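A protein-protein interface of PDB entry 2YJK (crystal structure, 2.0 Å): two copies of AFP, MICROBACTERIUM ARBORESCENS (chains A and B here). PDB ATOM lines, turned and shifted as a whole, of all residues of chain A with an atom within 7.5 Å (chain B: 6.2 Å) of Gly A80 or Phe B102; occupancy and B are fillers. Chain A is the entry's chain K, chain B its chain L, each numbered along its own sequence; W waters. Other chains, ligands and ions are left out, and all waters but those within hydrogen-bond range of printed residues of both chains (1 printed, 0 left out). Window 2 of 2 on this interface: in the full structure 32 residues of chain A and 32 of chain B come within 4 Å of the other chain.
The backbone carbonyl oxygen (O) of Ile A83 lies close to the backbone carbonyl oxygen (O) of Ala B100 (3.2 Å). The backbone carbonyl oxygen of Ile A83 lies within hydrogen-bond range of the side-chain amide nitrogen of Asn B45 (2.9 Å).
The backbone NH (N) of Arg B47 sits at hydrogen-bond distance from the backbone carbonyl oxygen (O) of Ala B103 (2.9 Å). O of Asn B45 sits at hydrogen-bond distance from N of Ala B103 (3.2 Å). The backbone carbonyl oxygen (O) of Ile A76 sits at hydrogen-bond distance from the backbone NH (N) of Leu A81, at 3.3 Å.
Glu A74 touches Trp B44 (OE2 to CD1, 3.4 Å). Val A77 touches Trp B44. CG1 of Val A77 touches NH2 of Arg B47, at 3.9 Å. Phe B102 touches Val A77. O of Gly A80 touches CE2 of Phe B102, at 3.5 Å. Phe B102 touches Leu A81. OD1 of Asn B45 touches CA of Pro A82 (3.5 Å). Gly B101 touches Pro A82. Pro A82 touches Phe B102.
Gly A80 touches just one residue of chain B: Phe B102 (3.5 Å). Of the printed residues of chain A, Trp B44 touches Glu A74 (3.4 Å) and Val A77 (3.6 Å). Of the printed residues of chain B, Glu A74 touches Trp B44 (3.4 Å). Of the printed residues of chain A, Ala B100 touches Ile A83. Printed residues of chain B within 4 Å of Ile A83: Asn B45 and Ala B100. Glu B108 touches none of the printed residues of chain A. Ala A10 touches none of the printed residues of chain B. The nearest residue of chain A that does not touch Phe B102 is Ile A83 (5.4 Å). The nearest printed residue of chain B that does not touch Leu A81 is Asn B45 (5.1 Å).
Printed residues of chain A that touch a printed residue of chain B: Glu A74, Val A77, Gly A80, Leu A81, Pro A82 and Ile A83. Hydrophobic or aromatic side chains of chain A within 4 Å of the printed part of chain B: Val A77, Pro A82 and Ile A83. Among the printed residues, 11 pairs touch across the chains.
No position is printed for both chains.
Water W1 bridges the guanidinium group of Arg B47 and the backbone carbonyl oxygen of Val A77.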
ATOM      1  N   ALA A  10      21.614 -23.707  16.911  1.00  0.00           N
ATOM      2  CA  ALA A  10      23.076 -24.027  17.055  1.00  0.00           C
ATOM      3  C   ALA A  10      23.921 -23.086  18.019  1.00  0.00           C
ATOM      4  O   ALA A  10      23.350 -22.342  18.865  1.00  0.00           O
ATOM      5  CB  ALA A  10      23.739 -24.161  15.625  1.00  0.00           C
ATOM      6  N   ALA A  18      16.861 -20.260  23.848  1.00  0.00           N
ATOM      7  CA  ALA A  18      16.132 -21.312  23.148  1.00  0.00           C
ATOM      8  C   ALA A  18      15.198 -22.055  24.114  1.00  0.00           C
ATOM      9  O   ALA A  18      14.028 -22.158  23.792  1.00  0.00           O
ATOM     10  CB  ALA A  18      17.081 -22.282  22.417  1.00  0.00           C
ATOM     11  N   GLU A  74       8.033 -21.805  14.023  1.00  0.00           N
ATOM     12  CA  GLU A  74       9.276 -21.494  13.318  1.00  0.00           C
ATOM     13  C   GLU A  74      10.218 -20.645  14.123  1.00  0.00           C
ATOM     14  O   GLU A  74      11.467 -20.682  13.901  1.00  0.00           O
ATOM     15  CB  GLU A  74       9.015 -20.917  11.925  1.00  0.00           C
ATOM     16  CG  GLU A  74       8.161 -21.935  11.237  1.00  0.00           C
ATOM     17  CD  GLU A  74       7.977 -21.718   9.742  1.00  0.00           C
ATOM     18  OE1 GLU A  74       8.000 -20.551   9.292  1.00  0.00           O
ATOM     19  OE2 GLU A  74       7.730 -22.740   9.042  1.00  0.00           O
ATOM     20  N   ARG A  75       9.651 -19.904  15.068  1.00  0.00           N
ATOM     21  CA  ARG A  75      10.486 -19.209  16.028  1.00  0.00           C
ATOM     22  C   ARG A  75      11.226 -20.209  16.921  1.00  0.00           C
ATOM     23  O   ARG A  75      12.460 -20.125  17.044  1.00  0.00           O
ATOM     24  CB  ARG A  75       9.662 -18.226  16.843  1.00  0.00           C
ATOM     25  CG  ARG A  75      10.456 -17.442  17.835  1.00  0.00           C
ATOM     26  CD  ARG A  75      11.595 -16.692  17.123  1.00  0.00           C
ATOM     27  NE  ARG A  75      12.458 -16.097  18.117  1.00  0.00           N
ATOM     28  CZ  ARG A  75      13.590 -15.451  17.845  1.00  0.00           C
ATOM     29  NH1 ARG A  75      13.979 -15.296  16.584  1.00  0.00           N
ATOM     30  NH2 ARG A  75      14.338 -14.986  18.834  1.00  0.00           N
ATOM     31  N   ILE A  76      10.512 -21.209  17.452  1.00  0.00           N
ATOM     32  CA  ILE A  76      11.169 -22.273  18.250  1.00  0.00           C
ATOM     33  C   ILE A  76      12.288 -22.993  17.432  1.00  0.00           C
ATOM     34  O   ILE A  76      13.443 -23.130  17.882  1.00  0.00           O
ATOM     35  CB  ILE A  76      10.118 -23.310  18.792  1.00  0.00           C
ATOM     36  CG1 ILE A  76       9.153 -22.597  19.776  1.00  0.00           C
ATOM     37  CG2 ILE A  76      10.789 -24.518  19.511  1.00  0.00           C
ATOM     38  CD1 ILE A  76       7.829 -23.258  19.820  1.00  0.00           C
ATOM     39  N   VAL A  77      11.930 -23.468  16.227  1.00  0.00           N
ATOM     40  CA  VAL A  77      12.869 -24.216  15.417  1.00  0.00           C
ATOM     41  C   VAL A  77      14.070 -23.341  14.990  1.00  0.00           C
ATOM     42  O   VAL A  77      15.198 -23.835  14.949  1.00  0.00           O
ATOM     43  CB  VAL A  77      12.203 -24.799  14.206  1.00  0.00           C
ATOM     44  CG1 VAL A  77      13.299 -25.443  13.322  1.00  0.00           C
ATOM     45  CG2 VAL A  77      11.151 -25.864  14.680  1.00  0.00           C
ATOM     46  N   ALA A  78      13.826 -22.058  14.694  1.00  0.00           N
ATOM     47  CA  ALA A  78      14.923 -21.115  14.356  1.00  0.00           C
ATOM     48  C   ALA A  78      15.980 -21.004  15.472  1.00  0.00           C
ATOM     49  O   ALA A  78      17.194 -20.827  15.202  1.00  0.00           O
ATOM     50  CB  ALA A  78      14.353 -19.693  13.983  1.00  0.00           C
ATOM     51  N   LEU A  79      15.514 -21.085  16.710  1.00  0.00           N
ATOM     52  CA  LEU A  79      16.393 -20.997  17.881  1.00  0.00           C
ATOM     53  C   LEU A  79      17.098 -22.325  18.139  1.00  0.00           C
ATOM     54  O   LEU A  79      17.854 -22.427  19.083  1.00  0.00           O
ATOM     55  CB  LEU A  79      15.586 -20.555  19.102  1.00  0.00           C
ATOM     56  CG  LEU A  79      15.117 -19.096  19.025  1.00  0.00           C
ATOM     57  CD1 LEU A  79      14.114 -18.754  20.118  1.00  0.00           C
ATOM     58  CD2 LEU A  79      16.313 -18.170  19.183  1.00  0.00           C
ATOM     59  N   GLY A  80      16.851 -23.339  17.286  1.00  0.00           N
ATOM     60  CA  GLY A  80      17.582 -24.597  17.384  1.00  0.00           C
ATOM     61  C   GLY A  80      16.882 -25.742  18.107  1.00  0.00           C
ATOM     62  O   GLY A  80      17.467 -26.790  18.226  1.00  0.00           O
ATOM     63  N   LEU A  81      15.632 -25.567  18.564  1.00  0.00           N
ATOM     64  CA  LEU A  81      14.908 -26.661  19.222  1.00  0.00           C
ATOM     65  C   LEU A  81      13.741 -27.318  18.433  1.00  0.00           C
ATOM     66  O   LEU A  81      13.093 -26.664  17.599  1.00  0.00           O
ATOM     67  CB  LEU A  81      14.414 -26.203  20.591  1.00  0.00           C
ATOM     68  CG  LEU A  81      15.470 -26.045  21.730  1.00  0.00           C
ATOM     69  CD1 LEU A  81      14.743 -25.674  23.045  1.00  0.00           C
ATOM     70  CD2 LEU A  81      16.396 -27.285  21.968  1.00  0.00           C
ATOM     71  N   PRO A  82      13.504 -28.634  18.662  1.00  0.00           N
ATOM     72  CA  PRO A  82      12.440 -29.329  17.942  1.00  0.00           C
ATOM     73  C   PRO A  82      11.061 -28.939  18.491  1.00  0.00           C
ATOM     74  O   PRO A  82      10.956 -28.336  19.567  1.00  0.00           O
ATOM     75  CB  PRO A  82      12.743 -30.788  18.254  1.00  0.00           C
ATOM     76  CG  PRO A  82      13.346 -30.715  19.680  1.00  0.00           C
ATOM     77  CD  PRO A  82      14.291 -29.583  19.505  1.00  0.00           C
ATOM     78  N   ILE A  83      10.002 -29.274  17.770  1.00  0.00           N
ATOM     79  CA  ILE A  83       8.657 -29.036  18.267  1.00  0.00           C
ATOM     80  C   ILE A  83       7.881 -30.333  18.003  1.00  0.00           C
ATOM     81  O   ILE A  83       7.940 -30.865  16.893  1.00  0.00           O
ATOM     82  CB  ILE A  83       8.030 -27.741  17.624  1.00  0.00           C
ATOM     83  CG1 ILE A  83       6.539 -27.645  17.903  1.00  0.00           C
ATOM     84  CG2 ILE A  83       8.178 -27.691  16.073  1.00  0.00           C
ATOM     85  CD1 ILE A  83       6.197 -27.155  19.309  1.00  0.00           C
ATOM     86  N   TRP B  44       8.120 -28.202   9.780  1.00  0.00           N
ATOM     87  CA  TRP B  44       8.902 -27.481  10.776  1.00  0.00           C
ATOM     88  C   TRP B  44      10.242 -28.195  11.103  1.00  0.00           C
ATOM     89  O   TRP B  44      11.284 -27.557  11.200  1.00  0.00           O
ATOM     90  CB  TRP B  44       8.065 -27.310  12.073  1.00  0.00           C
ATOM     91  CG  TRP B  44       6.823 -26.389  11.822  1.00  0.00           C
ATOM     92  CD1 TRP B  44       6.761 -25.316  10.979  1.00  0.00           C
ATOM     93  CD2 TRP B  44       5.541 -26.482  12.444  1.00  0.00           C
ATOM     94  NE1 TRP B  44       5.509 -24.779  11.002  1.00  0.00           N
ATOM     95  CE2 TRP B  44       4.739 -25.466  11.894  1.00  0.00           C
ATOM     96  CE3 TRP B  44       4.992 -27.343  13.401  1.00  0.00           C
ATOM     97  CZ2 TRP B  44       3.413 -25.226  12.310  1.00  0.00           C
ATOM     98  CZ3 TRP B  44       3.679 -27.172  13.764  1.00  0.00           C
ATOM     99  CH2 TRP B  44       2.882 -26.087  13.212  1.00  0.00           C
ATOM    100  N   ASN B  45      10.187 -29.510  11.261  1.00  0.00           N
ATOM    101  CA  ASN B  45      11.279 -30.241  11.865  1.00  0.00           C
ATOM    102  C   ASN B  45      12.212 -30.864  10.874  1.00  0.00           C
ATOM    103  O   ASN B  45      13.168 -31.498  11.311  1.00  0.00           O
ATOM    104  CB  ASN B  45      10.720 -31.358  12.794  1.00  0.00           C
ATOM    105  CG  ASN B  45      10.123 -30.790  14.061  1.00  0.00           C
ATOM    106  OD1 ASN B  45      10.846 -30.444  14.985  1.00  0.00           O
ATOM    107  ND2 ASN B  45       8.791 -30.647  14.094  1.00  0.00           N
ATOM    108  N   VAL B  46      11.924 -30.763   9.559  1.00  0.00           N
ATOM    109  CA  VAL B  46      12.769 -31.400   8.499  1.00  0.00           C
ATOM    110  C   VAL B  46      14.203 -30.802   8.451  1.00  0.00           C
ATOM    111  O   VAL B  46      14.361 -29.635   8.685  1.00  0.00           O
ATOM    112  CB  VAL B  46      12.080 -31.363   7.073  1.00  0.00           C
ATOM    113  CG1 VAL B  46      11.805 -29.915   6.563  1.00  0.00           C
ATOM    114  CG2 VAL B  46      12.879 -32.155   6.051  1.00  0.00           C
ATOM    115  N   ARG B  47      15.238 -31.627   8.192  1.00  0.00           N
ATOM    116  CA  ARG B  47      16.633 -31.148   8.111  1.00  0.00           C
ATOM    117  C   ARG B  47      17.418 -31.796   6.951  1.00  0.00           C
ATOM    118  O   ARG B  47      16.980 -32.803   6.390  1.00  0.00           O
ATOM    119  CB  ARG B  47      17.391 -31.496   9.381  1.00  0.00           C
ATOM    120  CG  ARG B  47      16.607 -31.376  10.663  1.00  0.00           C
ATOM    121  CD  ARG B  47      17.474 -30.571  11.597  1.00  0.00           C
ATOM    122  NE  ARG B  47      16.915 -29.260  11.535  1.00  0.00           N
ATOM    123  CZ  ARG B  47      17.281 -28.221  12.288  1.00  0.00           C
ATOM    124  NH1 ARG B  47      18.254 -28.337  13.197  1.00  0.00           N
ATOM    125  NH2 ARG B  47      16.616 -27.065  12.119  1.00  0.00           N
ATOM    126  N   PRO B  99       8.061 -38.241  12.749  1.00  0.00           N
ATOM    127  CA  PRO B  99       8.788 -38.232  14.064  1.00  0.00           C
ATOM    128  C   PRO B  99       8.418 -37.070  14.956  1.00  0.00           C
ATOM    129  O   PRO B  99       7.898 -36.029  14.509  1.00  0.00           O
ATOM    130  CB  PRO B  99      10.279 -38.163  13.706  1.00  0.00           C
ATOM    131  CG  PRO B  99      10.369 -38.460  12.188  1.00  0.00           C
ATOM    132  CD  PRO B  99       8.979 -38.323  11.578  1.00  0.00           C
ATOM    133  N   ALA B 100       8.726 -37.256  16.221  1.00  0.00           N
ATOM    134  CA  ALA B 100       8.377 -36.282  17.267  1.00  0.00           C
ATOM    135  C   ALA B 100       9.204 -34.989  17.163  1.00  0.00           C
ATOM    136  O   ALA B 100       8.737 -33.931  17.599  1.00  0.00           O
ATOM    137  CB  ALA B 100       8.573 -36.947  18.677  1.00  0.00           C
ATOM    138  N   GLY B 101      10.422 -35.088  16.619  1.00  0.00           N
ATOM    139  CA  GLY B 101      11.327 -33.947  16.489  1.00  0.00           C
ATOM    140  C   GLY B 101      12.084 -33.876  15.160  1.00  0.00           C
ATOM    141  O   GLY B 101      11.583 -34.282  14.082  1.00  0.00           O
ATOM    142  N   PHE B 102      13.322 -33.429  15.239  1.00  0.00           N
ATOM    143  CA  PHE B 102      14.102 -33.190  14.051  1.00  0.00           C
ATOM    144  C   PHE B 102      14.323 -34.467  13.327  1.00  0.00           C
ATOM    145  O   PHE B 102      14.564 -35.496  13.984  1.00  0.00           O
ATOM    146  CB  PHE B 102      15.464 -32.640  14.439  1.00  0.00           C
ATOM    147  CG  PHE B 102      15.430 -31.191  14.863  1.00  0.00           C
ATOM    148  CD1 PHE B 102      14.506 -30.285  14.280  1.00  0.00           C
ATOM    149  CD2 PHE B 102      16.372 -30.708  15.738  1.00  0.00           C
ATOM    150  CE1 PHE B 102      14.454 -28.945  14.656  1.00  0.00           C
ATOM    151  CE2 PHE B 102      16.330 -29.360  16.113  1.00  0.00           C
ATOM    152  CZ  PHE B 102      15.381 -28.476  15.563  1.00  0.00           C
ATOM    153  N   ALA B 103      14.240 -34.419  11.999  1.00  0.00           N
ATOM    154  CA  ALA B 103      14.476 -35.621  11.216  1.00  0.00           C
ATOM    155  C   ALA B 103      15.042 -35.283   9.846  1.00  0.00           C
ATOM    156  O   ALA B 103      14.702 -34.284   9.263  1.00  0.00           O
ATOM    157  CB  ALA B 103      13.161 -36.486  11.058  1.00  0.00           C
ATOM    158  N   GLN B 104      15.883 -36.165   9.338  1.00  0.00           N
ATOM    159  CA  GLN B 104      16.465 -36.000   7.993  1.00  0.00           C
ATOM    160  C   GLN B 104      15.349 -36.003   6.970  1.00  0.00           C
ATOM    161  O   GLN B 104      14.329 -36.681   7.159  1.00  0.00           O
ATOM    162  CB  GLN B 104      17.499 -37.109   7.741  1.00  0.00           C
ATOM    163  CG  GLN B 104      18.766 -36.917   8.517  1.00  0.00           C
ATOM    164  CD  GLN B 104      19.464 -35.573   8.190  1.00  0.00           C
ATOM    165  OE1 GLN B 104      19.631 -34.673   9.065  1.00  0.00           O
ATOM    166  NE2 GLN B 104      19.866 -35.433   6.940  1.00  0.00           N
ATOM    167  N   GLU B 108      11.456 -37.848   6.632  1.00  0.00           N
ATOM    168  CA  GLU B 108      10.200 -37.077   6.674  1.00  0.00           C
ATOM    169  C   GLU B 108       9.350 -37.534   5.453  1.00  0.00           C
ATOM    170  O   GLU B 108       8.151 -37.744   5.590  1.00  0.00           O
ATOM    171  CB  GLU B 108      10.438 -35.545   6.629  1.00  0.00           C
ATOM    172  CG  GLU B 108      11.101 -34.950   7.903  1.00  0.00           C
ATOM    173  CD  GLU B 108      10.219 -35.050   9.154  1.00  0.00           C
ATOM    174  OE1 GLU B 108       9.148 -35.692   9.090  1.00  0.00           O
ATOM    175  OE2 GLU B 108      10.580 -34.479  10.211  1.00  0.00           O
HETATM  176  O   HOH W   1      17.284 -25.315  13.714  1.00  0.00           O
